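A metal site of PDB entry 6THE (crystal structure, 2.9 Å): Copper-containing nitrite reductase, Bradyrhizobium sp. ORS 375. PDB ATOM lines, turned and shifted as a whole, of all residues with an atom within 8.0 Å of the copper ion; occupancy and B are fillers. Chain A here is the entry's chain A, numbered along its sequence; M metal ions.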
ATOM      1  N   SER A  35     -29.581 -34.665   6.705  1.00  0.00           N
ATOM      2  CA  SER A  35     -29.214 -33.269   6.837  1.00  0.00           C
ATOM      3  C   SER A  35     -30.467 -32.402   6.780  1.00  0.00           C
ATOM      4  O   SER A  35     -31.190 -32.404   5.779  1.00  0.00           O
ATOM      5  CB  SER A  35     -28.210 -32.867   5.788  1.00  0.00           C
ATOM      6  OG  SER A  35     -28.703 -33.099   4.484  1.00  0.00           O
ATOM      7  N   GLU A  37     -32.176 -28.456   7.671  1.00  0.00           N
ATOM      8  CA  GLU A  37     -32.040 -27.043   7.989  1.00  0.00           C
ATOM      9  C   GLU A  37     -33.312 -26.592   8.704  1.00  0.00           C
ATOM     10  O   GLU A  37     -34.407 -26.715   8.166  1.00  0.00           O
ATOM     11  CB  GLU A  37     -31.836 -26.221   6.712  1.00  0.00           C
ATOM     12  CG  GLU A  37     -30.673 -26.687   5.848  1.00  0.00           C
ATOM     13  CD  GLU A  37     -30.503 -25.925   4.546  1.00  0.00           C
ATOM     14  OE1 GLU A  37     -29.841 -26.471   3.637  1.00  0.00           O
ATOM     15  OE2 GLU A  37     -31.011 -24.798   4.442  1.00  0.00           O
ATOM     16  N   TRP A  51     -27.840 -25.553  10.154  1.00  0.00           N
ATOM     17  CA  TRP A  51     -27.720 -26.745   9.329  1.00  0.00           C
ATOM     18  C   TRP A  51     -27.230 -27.885  10.218  1.00  0.00           C
ATOM     19  O   TRP A  51     -26.200 -27.750  10.888  1.00  0.00           O
ATOM     20  CB  TRP A  51     -26.772 -26.502   8.140  1.00  0.00           C
ATOM     21  CG  TRP A  51     -27.079 -25.293   7.299  1.00  0.00           C
ATOM     22  CD1 TRP A  51     -28.272 -24.623   7.222  1.00  0.00           C
ATOM     23  CD2 TRP A  51     -26.191 -24.629   6.392  1.00  0.00           C
ATOM     24  NE1 TRP A  51     -28.168 -23.587   6.347  1.00  0.00           N
ATOM     25  CE2 TRP A  51     -26.904 -23.559   5.820  1.00  0.00           C
ATOM     26  CE3 TRP A  51     -24.848 -24.827   6.018  1.00  0.00           C
ATOM     27  CZ2 TRP A  51     -26.326 -22.697   4.886  1.00  0.00           C
ATOM     28  CZ3 TRP A  51     -24.287 -23.975   5.095  1.00  0.00           C
ATOM     29  CH2 TRP A  51     -25.022 -22.923   4.536  1.00  0.00           C
ATOM     30  N   THR A  52     -27.981 -28.988  10.238  1.00  0.00           N
ATOM     31  CA  THR A  52     -27.797 -30.020  11.247  1.00  0.00           C
ATOM     32  C   THR A  52     -27.720 -31.407  10.612  1.00  0.00           C
ATOM     33  O   THR A  52     -28.150 -31.610   9.484  1.00  0.00           O
ATOM     34  CB  THR A  52     -28.958 -30.020  12.253  1.00  0.00           C
ATOM     35  OG1 THR A  52     -30.156 -30.319  11.542  1.00  0.00           O
ATOM     36  CG2 THR A  52     -29.127 -28.701  12.985  1.00  0.00           C
ATOM     37  N   PHE A  53     -27.156 -32.351  11.377  1.00  0.00           N
ATOM     38  CA  PHE A  53     -27.295 -33.774  11.137  1.00  0.00           C
ATOM     39  C   PHE A  53     -28.311 -34.337  12.126  1.00  0.00           C
ATOM     40  O   PHE A  53     -28.048 -34.360  13.331  1.00  0.00           O
ATOM     41  CB  PHE A  53     -25.957 -34.501  11.296  1.00  0.00           C
ATOM     42  CG  PHE A  53     -24.947 -34.297  10.192  1.00  0.00           C
ATOM     43  CD1 PHE A  53     -25.159 -34.839   8.929  1.00  0.00           C
ATOM     44  CD2 PHE A  53     -23.771 -33.609  10.414  1.00  0.00           C
ATOM     45  CE1 PHE A  53     -24.225 -34.665   7.918  1.00  0.00           C
ATOM     46  CE2 PHE A  53     -22.837 -33.435   9.403  1.00  0.00           C
ATOM     47  CZ  PHE A  53     -23.061 -33.966   8.151  1.00  0.00           C
ATOM     48  N   LEU A  74     -26.548 -41.046   3.378  1.00  0.00           N
ATOM     49  CA  LEU A  74     -26.802 -39.636   3.616  1.00  0.00           C
ATOM     50  C   LEU A  74     -27.990 -39.175   2.773  1.00  0.00           C
ATOM     51  O   LEU A  74     -27.909 -39.114   1.549  1.00  0.00           O
ATOM     52  CB  LEU A  74     -25.535 -38.828   3.300  1.00  0.00           C
ATOM     53  CG  LEU A  74     -25.576 -37.359   3.729  1.00  0.00           C
ATOM     54  CD1 LEU A  74     -25.460 -37.221   5.235  1.00  0.00           C
ATOM     55  CD2 LEU A  74     -24.472 -36.568   3.037  1.00  0.00           C
ATOM     56  N   ASN A  76     -30.782 -36.049   2.146  1.00  0.00           N
ATOM     57  CA  ASN A  76     -30.970 -34.621   2.310  1.00  0.00           C
ATOM     58  C   ASN A  76     -32.466 -34.305   2.249  1.00  0.00           C
ATOM     59  O   ASN A  76     -33.160 -34.768   1.343  1.00  0.00           O
ATOM     60  CB  ASN A  76     -30.167 -33.817   1.278  1.00  0.00           C
ATOM     61  CG  ASN A  76     -29.937 -32.381   1.668  1.00  0.00           C
ATOM     62  OD1 ASN A  76     -30.400 -31.923   2.712  1.00  0.00           O
ATOM     63  ND2 ASN A  76     -29.211 -31.645   0.838  1.00  0.00           N
ATOM     64  N   MET A  82     -29.464 -26.169   0.592  1.00  0.00           N
ATOM     65  CA  MET A  82     -28.037 -26.341   0.349  1.00  0.00           C
ATOM     66  C   MET A  82     -27.725 -27.804   0.067  1.00  0.00           C
ATOM     67  O   MET A  82     -28.452 -28.702   0.482  1.00  0.00           O
ATOM     68  CB  MET A  82     -27.221 -25.891   1.568  1.00  0.00           C
ATOM     69  CG  MET A  82     -27.359 -24.404   1.898  1.00  0.00           C
ATOM     70  SD  MET A  82     -26.723 -23.316   0.600  1.00  0.00           S
ATOM     71  CE  MET A  82     -24.965 -23.591   0.747  1.00  0.00           C
ATOM     72  N   ILE A  83     -26.619 -28.025  -0.666  1.00  0.00           N
ATOM     73  CA  ILE A  83     -26.038 -29.339  -0.860  1.00  0.00           C
ATOM     74  C   ILE A  83     -25.284 -29.701   0.420  1.00  0.00           C
ATOM     75  O   ILE A  83     -24.611 -28.857   1.005  1.00  0.00           O
ATOM     76  CB  ILE A  83     -25.110 -29.348  -2.095  1.00  0.00           C
ATOM     77  CG1 ILE A  83     -25.824 -28.843  -3.354  1.00  0.00           C
ATOM     78  CG2 ILE A  83     -24.487 -30.721  -2.308  1.00  0.00           C
ATOM     79  CD1 ILE A  83     -24.905 -28.376  -4.452  1.00  0.00           C
ATOM     80  N   HIS A  84     -25.406 -30.964   0.842  1.00  0.00           N
ATOM     81  CA  HIS A  84     -24.777 -31.421   2.073  1.00  0.00           C
ATOM     82  C   HIS A  84     -23.974 -32.691   1.816  1.00  0.00           C
ATOM     83  O   HIS A  84     -24.312 -33.492   0.951  1.00  0.00           O
ATOM     84  CB  HIS A  84     -25.806 -31.585   3.187  1.00  0.00           C
ATOM     85  CG  HIS A  84     -26.494 -30.310   3.574  1.00  0.00           C
ATOM     86  ND1 HIS A  84     -25.793 -29.194   3.982  1.00  0.00           N
ATOM     87  CD2 HIS A  84     -27.801 -29.983   3.624  1.00  0.00           C
ATOM     88  CE1 HIS A  84     -26.651 -28.228   4.264  1.00  0.00           C
ATOM     89  NE2 HIS A  84     -27.882 -28.688   4.051  1.00  0.00           N
ATOM     90  N   SER A  85     -22.893 -32.853   2.594  1.00  0.00           N
ATOM     91  CA  SER A  85     -22.036 -34.024   2.557  1.00  0.00           C
ATOM     92  C   SER A  85     -21.617 -34.392   3.972  1.00  0.00           C
ATOM     93  O   SER A  85     -22.116 -33.824   4.937  1.00  0.00           O
ATOM     94  CB  SER A  85     -20.851 -33.793   1.655  1.00  0.00           C
ATOM     95  OG  SER A  85     -20.116 -32.644   2.081  1.00  0.00           O
ATOM     96  N   VAL A  86     -20.693 -35.356   4.089  1.00  0.00           N
ATOM     97  CA  VAL A  86     -20.129 -35.740   5.373  1.00  0.00           C
ATOM     98  C   VAL A  86     -18.714 -36.277   5.173  1.00  0.00           C
ATOM     99  O   VAL A  86     -18.490 -37.172   4.362  1.00  0.00           O
ATOM    100  CB  VAL A  86     -21.037 -36.705   6.162  1.00  0.00           C
ATOM    101  CG1 VAL A  86     -21.369 -37.975   5.395  1.00  0.00           C
ATOM    102  CG2 VAL A  86     -20.489 -37.023   7.536  1.00  0.00           C
ATOM    103  N   GLN A 102     -21.945 -35.958  -1.965  1.00  0.00           N
ATOM    104  CA  GLN A 102     -22.537 -34.662  -2.256  1.00  0.00           C
ATOM    105  C   GLN A 102     -23.998 -34.889  -2.641  1.00  0.00           C
ATOM    106  O   GLN A 102     -24.299 -35.267  -3.776  1.00  0.00           O
ATOM    107  CB  GLN A 102     -21.756 -33.939  -3.350  1.00  0.00           C
ATOM    108  CG  GLN A 102     -20.311 -33.635  -2.989  1.00  0.00           C
ATOM    109  CD  GLN A 102     -20.148 -32.607  -1.903  1.00  0.00           C
ATOM    110  OE1 GLN A 102     -20.957 -31.691  -1.747  1.00  0.00           O
ATOM    111  NE2 GLN A 102     -19.075 -32.730  -1.137  1.00  0.00           N
ATOM    112  N   VAL A 103     -24.899 -34.653  -1.680  1.00  0.00           N
ATOM    113  CA  VAL A 103     -26.307 -34.987  -1.832  1.00  0.00           C
ATOM    114  C   VAL A 103     -27.114 -33.696  -2.005  1.00  0.00           C
ATOM    115  O   VAL A 103     -27.047 -32.802  -1.178  1.00  0.00           O
ATOM    116  CB  VAL A 103     -26.819 -35.835  -0.651  1.00  0.00           C
ATOM    117  CG1 VAL A 103     -28.283 -36.212  -0.818  1.00  0.00           C
ATOM    118  CG2 VAL A 103     -25.978 -37.076  -0.444  1.00  0.00           C
ATOM    119  N   HIS A 124     -17.909 -34.008   9.724  1.00  0.00           N
ATOM    120  CA  HIS A 124     -18.497 -32.721   9.377  1.00  0.00           C
ATOM    121  C   HIS A 124     -18.867 -32.707   7.895  1.00  0.00           C
ATOM    122  O   HIS A 124     -18.397 -33.528   7.123  1.00  0.00           O
ATOM    123  CB  HIS A 124     -17.550 -31.572   9.739  1.00  0.00           C
ATOM    124  CG  HIS A 124     -16.210 -31.668   9.065  1.00  0.00           C
ATOM    125  ND1 HIS A 124     -15.971 -31.134   7.820  1.00  0.00           N
ATOM    126  CD2 HIS A 124     -15.050 -32.231   9.472  1.00  0.00           C
ATOM    127  CE1 HIS A 124     -14.724 -31.370   7.475  1.00  0.00           C
ATOM    128  NE2 HIS A 124     -14.134 -32.040   8.478  1.00  0.00           N
ATOM    129  N   CYS A 125     -19.720 -31.741   7.516  1.00  0.00           N
ATOM    130  CA  CYS A 125     -20.074 -31.507   6.127  1.00  0.00           C
ATOM    131  C   CYS A 125     -18.876 -30.902   5.403  1.00  0.00           C
ATOM    132  O   CYS A 125     -18.207 -30.010   5.935  1.00  0.00           O
ATOM    133  CB  CYS A 125     -21.274 -30.564   6.030  1.00  0.00           C
ATOM    134  SG  CYS A 125     -21.870 -30.318   4.345  1.00  0.00           S
ATOM    135  N   ALA A 126     -18.627 -31.378   4.176  1.00  0.00           N
ATOM    136  CA  ALA A 126     -17.501 -30.924   3.375  1.00  0.00           C
ATOM    137  C   ALA A 126     -17.998 -30.407   2.025  1.00  0.00           C
ATOM    138  O   ALA A 126     -17.497 -30.828   0.983  1.00  0.00           O
ATOM    139  CB  ALA A 126     -16.487 -32.037   3.227  1.00  0.00           C
ATOM    140  N   THR A 127     -18.978 -29.502   2.069  1.00  0.00           N
ATOM    141  CA  THR A 127     -19.521 -28.863   0.881  1.00  0.00           C
ATOM    142  C   THR A 127     -19.104 -27.398   0.872  1.00  0.00           C
ATOM    143  O   THR A 127     -19.253 -26.721   1.891  1.00  0.00           O
ATOM    144  CB  THR A 127     -21.042 -29.045   0.809  1.00  0.00           C
ATOM    145  OG1 THR A 127     -21.336 -30.430   0.969  1.00  0.00           O
ATOM    146  CG2 THR A 127     -21.641 -28.543  -0.489  1.00  0.00           C
ATOM    147  N   PRO A 128     -18.552 -26.876  -0.236  1.00  0.00           N
ATOM    148  CA  PRO A 128     -18.176 -25.464  -0.339  1.00  0.00           C
ATOM    149  C   PRO A 128     -19.316 -24.495  -0.015  1.00  0.00           C
ATOM    150  O   PRO A 128     -20.421 -24.640  -0.524  1.00  0.00           O
ATOM    151  CB  PRO A 128     -17.755 -25.301  -1.811  1.00  0.00           C
ATOM    152  CG  PRO A 128     -17.282 -26.684  -2.203  1.00  0.00           C
ATOM    153  CD  PRO A 128     -18.211 -27.625  -1.459  1.00  0.00           C
ATOM    154  N   MET A 129     -19.037 -23.522   0.878  1.00  0.00           N
ATOM    155  CA  MET A 129     -17.755 -23.452   1.556  1.00  0.00           C
ATOM    156  C   MET A 129     -17.850 -24.172   2.909  1.00  0.00           C
ATOM    157  O   MET A 129     -18.832 -24.010   3.636  1.00  0.00           O
ATOM    158  CB  MET A 129     -17.244 -22.015   1.724  1.00  0.00           C
ATOM    159  CG  MET A 129     -18.075 -21.139   2.649  1.00  0.00           C
ATOM    160  SD  MET A 129     -17.124 -19.729   3.277  1.00  0.00           S
ATOM    161  CE  MET A 129     -17.099 -18.672   1.825  1.00  0.00           C
ATOM    162  N   VAL A 130     -16.818 -24.961   3.206  1.00  0.00           N
ATOM    163  CA  VAL A 130     -16.830 -25.978   4.244  1.00  0.00           C
ATOM    164  C   VAL A 130     -16.943 -25.319   5.618  1.00  0.00           C
ATOM    165  O   VAL A 130     -17.630 -25.840   6.497  1.00  0.00           O
ATOM    166  CB  VAL A 130     -15.598 -26.898   4.140  1.00  0.00           C
ATOM    167  CG1 VAL A 130     -15.601 -27.986   5.209  1.00  0.00           C
ATOM    168  CG2 VAL A 130     -15.465 -27.511   2.759  1.00  0.00           C
ATOM    169  N   GLU A 132     -18.464 -22.684   6.471  1.00  0.00           N
ATOM    170  CA  GLU A 132     -19.824 -22.210   6.705  1.00  0.00           C
ATOM    171  C   GLU A 132     -20.712 -23.371   7.170  1.00  0.00           C
ATOM    172  O   GLU A 132     -21.465 -23.222   8.127  1.00  0.00           O
ATOM    173  CB  GLU A 132     -20.381 -21.562   5.441  1.00  0.00           C
ATOM    174  CG  GLU A 132     -21.836 -21.129   5.550  1.00  0.00           C
ATOM    175  CD  GLU A 132     -22.421 -20.493   4.304  1.00  0.00           C
ATOM    176  OE1 GLU A 132     -23.381 -19.704   4.452  1.00  0.00           O
ATOM    177  OE2 GLU A 132     -21.933 -20.791   3.194  1.00  0.00           O
ATOM    178  N   HIS A 133     -20.589 -24.519   6.480  1.00  0.00           N
ATOM    179  CA  HIS A 133     -21.415 -25.687   6.753  1.00  0.00           C
ATOM    180  C   HIS A 133     -21.140 -26.210   8.162  1.00  0.00           C
ATOM    181  O   HIS A 133     -22.076 -26.612   8.860  1.00  0.00           O
ATOM    182  CB  HIS A 133     -21.206 -26.752   5.663  1.00  0.00           C
ATOM    183  CG  HIS A 133     -21.873 -26.413   4.374  1.00  0.00           C
ATOM    184  ND1 HIS A 133     -23.017 -27.054   3.943  1.00  0.00           N
ATOM    185  CD2 HIS A 133     -21.569 -25.499   3.422  1.00  0.00           C
ATOM    186  CE1 HIS A 133     -23.386 -26.550   2.772  1.00  0.00           C
ATOM    187  NE2 HIS A 133     -22.513 -25.599   2.434  1.00  0.00           N
ATOM    188  N   ILE A 134     -19.867 -26.189   8.565  1.00  0.00           N
ATOM    189  CA  ILE A 134     -19.466 -26.610   9.894  1.00  0.00           C
ATOM    190  C   ILE A 134     -20.027 -25.631  10.923  1.00  0.00           C
ATOM    191  O   ILE A 134     -20.640 -26.041  11.906  1.00  0.00           O
ATOM    192  CB  ILE A 134     -17.930 -26.753   9.996  1.00  0.00           C
ATOM    193  CG1 ILE A 134     -17.397 -27.838   9.047  1.00  0.00           C
ATOM    194  CG2 ILE A 134     -17.504 -27.017  11.437  1.00  0.00           C
ATOM    195  CD1 ILE A 134     -15.888 -27.824   8.890  1.00  0.00           C
ATOM    196  N   ASN A 136     -22.479 -23.731  10.888  1.00  0.00           N
ATOM    197  CA  ASN A 136     -23.933 -23.725  10.992  1.00  0.00           C
ATOM    198  C   ASN A 136     -24.420 -24.948  11.772  1.00  0.00           C
ATOM    199  O   ASN A 136     -25.596 -25.058  12.085  1.00  0.00           O
ATOM    200  CB  ASN A 136     -24.598 -23.500   9.628  1.00  0.00           C
ATOM    201  CG  ASN A 136     -24.382 -22.106   9.080  1.00  0.00           C
ATOM    202  OD1 ASN A 136     -24.082 -21.181   9.832  1.00  0.00           O
ATOM    203  ND2 ASN A 136     -24.544 -21.944   7.785  1.00  0.00           N
ATOM    204  N   GLY A 137     -23.486 -25.867  12.083  1.00  0.00           N
ATOM    205  CA  GLY A 137     -23.725 -26.897  13.078  1.00  0.00           C
ATOM    206  C   GLY A 137     -23.551 -28.316  12.541  1.00  0.00           C
ATOM    207  O   GLY A 137     -23.879 -29.276  13.233  1.00  0.00           O
ATOM    208  N   MET A 138     -23.016 -28.444  11.323  1.00  0.00           N
ATOM    209  CA  MET A 138     -22.867 -29.751  10.698  1.00  0.00           C
ATOM    210  C   MET A 138     -21.515 -30.351  11.076  1.00  0.00           C
ATOM    211  O   MET A 138     -20.583 -30.354  10.277  1.00  0.00           O
ATOM    212  CB  MET A 138     -22.987 -29.668   9.174  1.00  0.00           C
ATOM    213  CG  MET A 138     -24.349 -29.178   8.705  1.00  0.00           C
ATOM    214  SD  MET A 138     -24.611 -29.385   6.928  1.00  0.00           S
ATOM    215  CE  MET A 138     -25.014 -31.123   6.861  1.00  0.00           C
HETATM  216 CU    CU M   1     -23.638 -28.976   4.682  1.00  0.00          CU
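A ring nitrogen (NE2) of His 133 lies close to the backbone carbonyl oxygen (O) of Thr 127 (3.5 Å). SG of Cys 125 lies close to N of Ser 85 (3.2 Å). SG of Cys 125 lies close to OG1 of Thr 127. A ring nitrogen (NE2) of His 84 lies within hydrogen-bond range of the side-chain carboxylate (OE1) of Glu 37 (3.0 Å). The backbone carbonyl oxygen (O) of His 84 lies within hydrogen-bond range of the backbone NH (N) of Val 103 (2.9 Å). N of Met 138 lies close to O of Trp 51 (3.3 Å).
Residues that only touch the copper ion: Ile 83 (3.8 Å). Of the 27 residues printed, 5 come within 4 Å of the copper ion.
The copper ion is bound by ND1 of His 133 (2.2 Å), SG of Cys 125 (2.2 Å), ND1 of His 84 (2.3 Å) and SD of Met 138 (2.5 Å).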
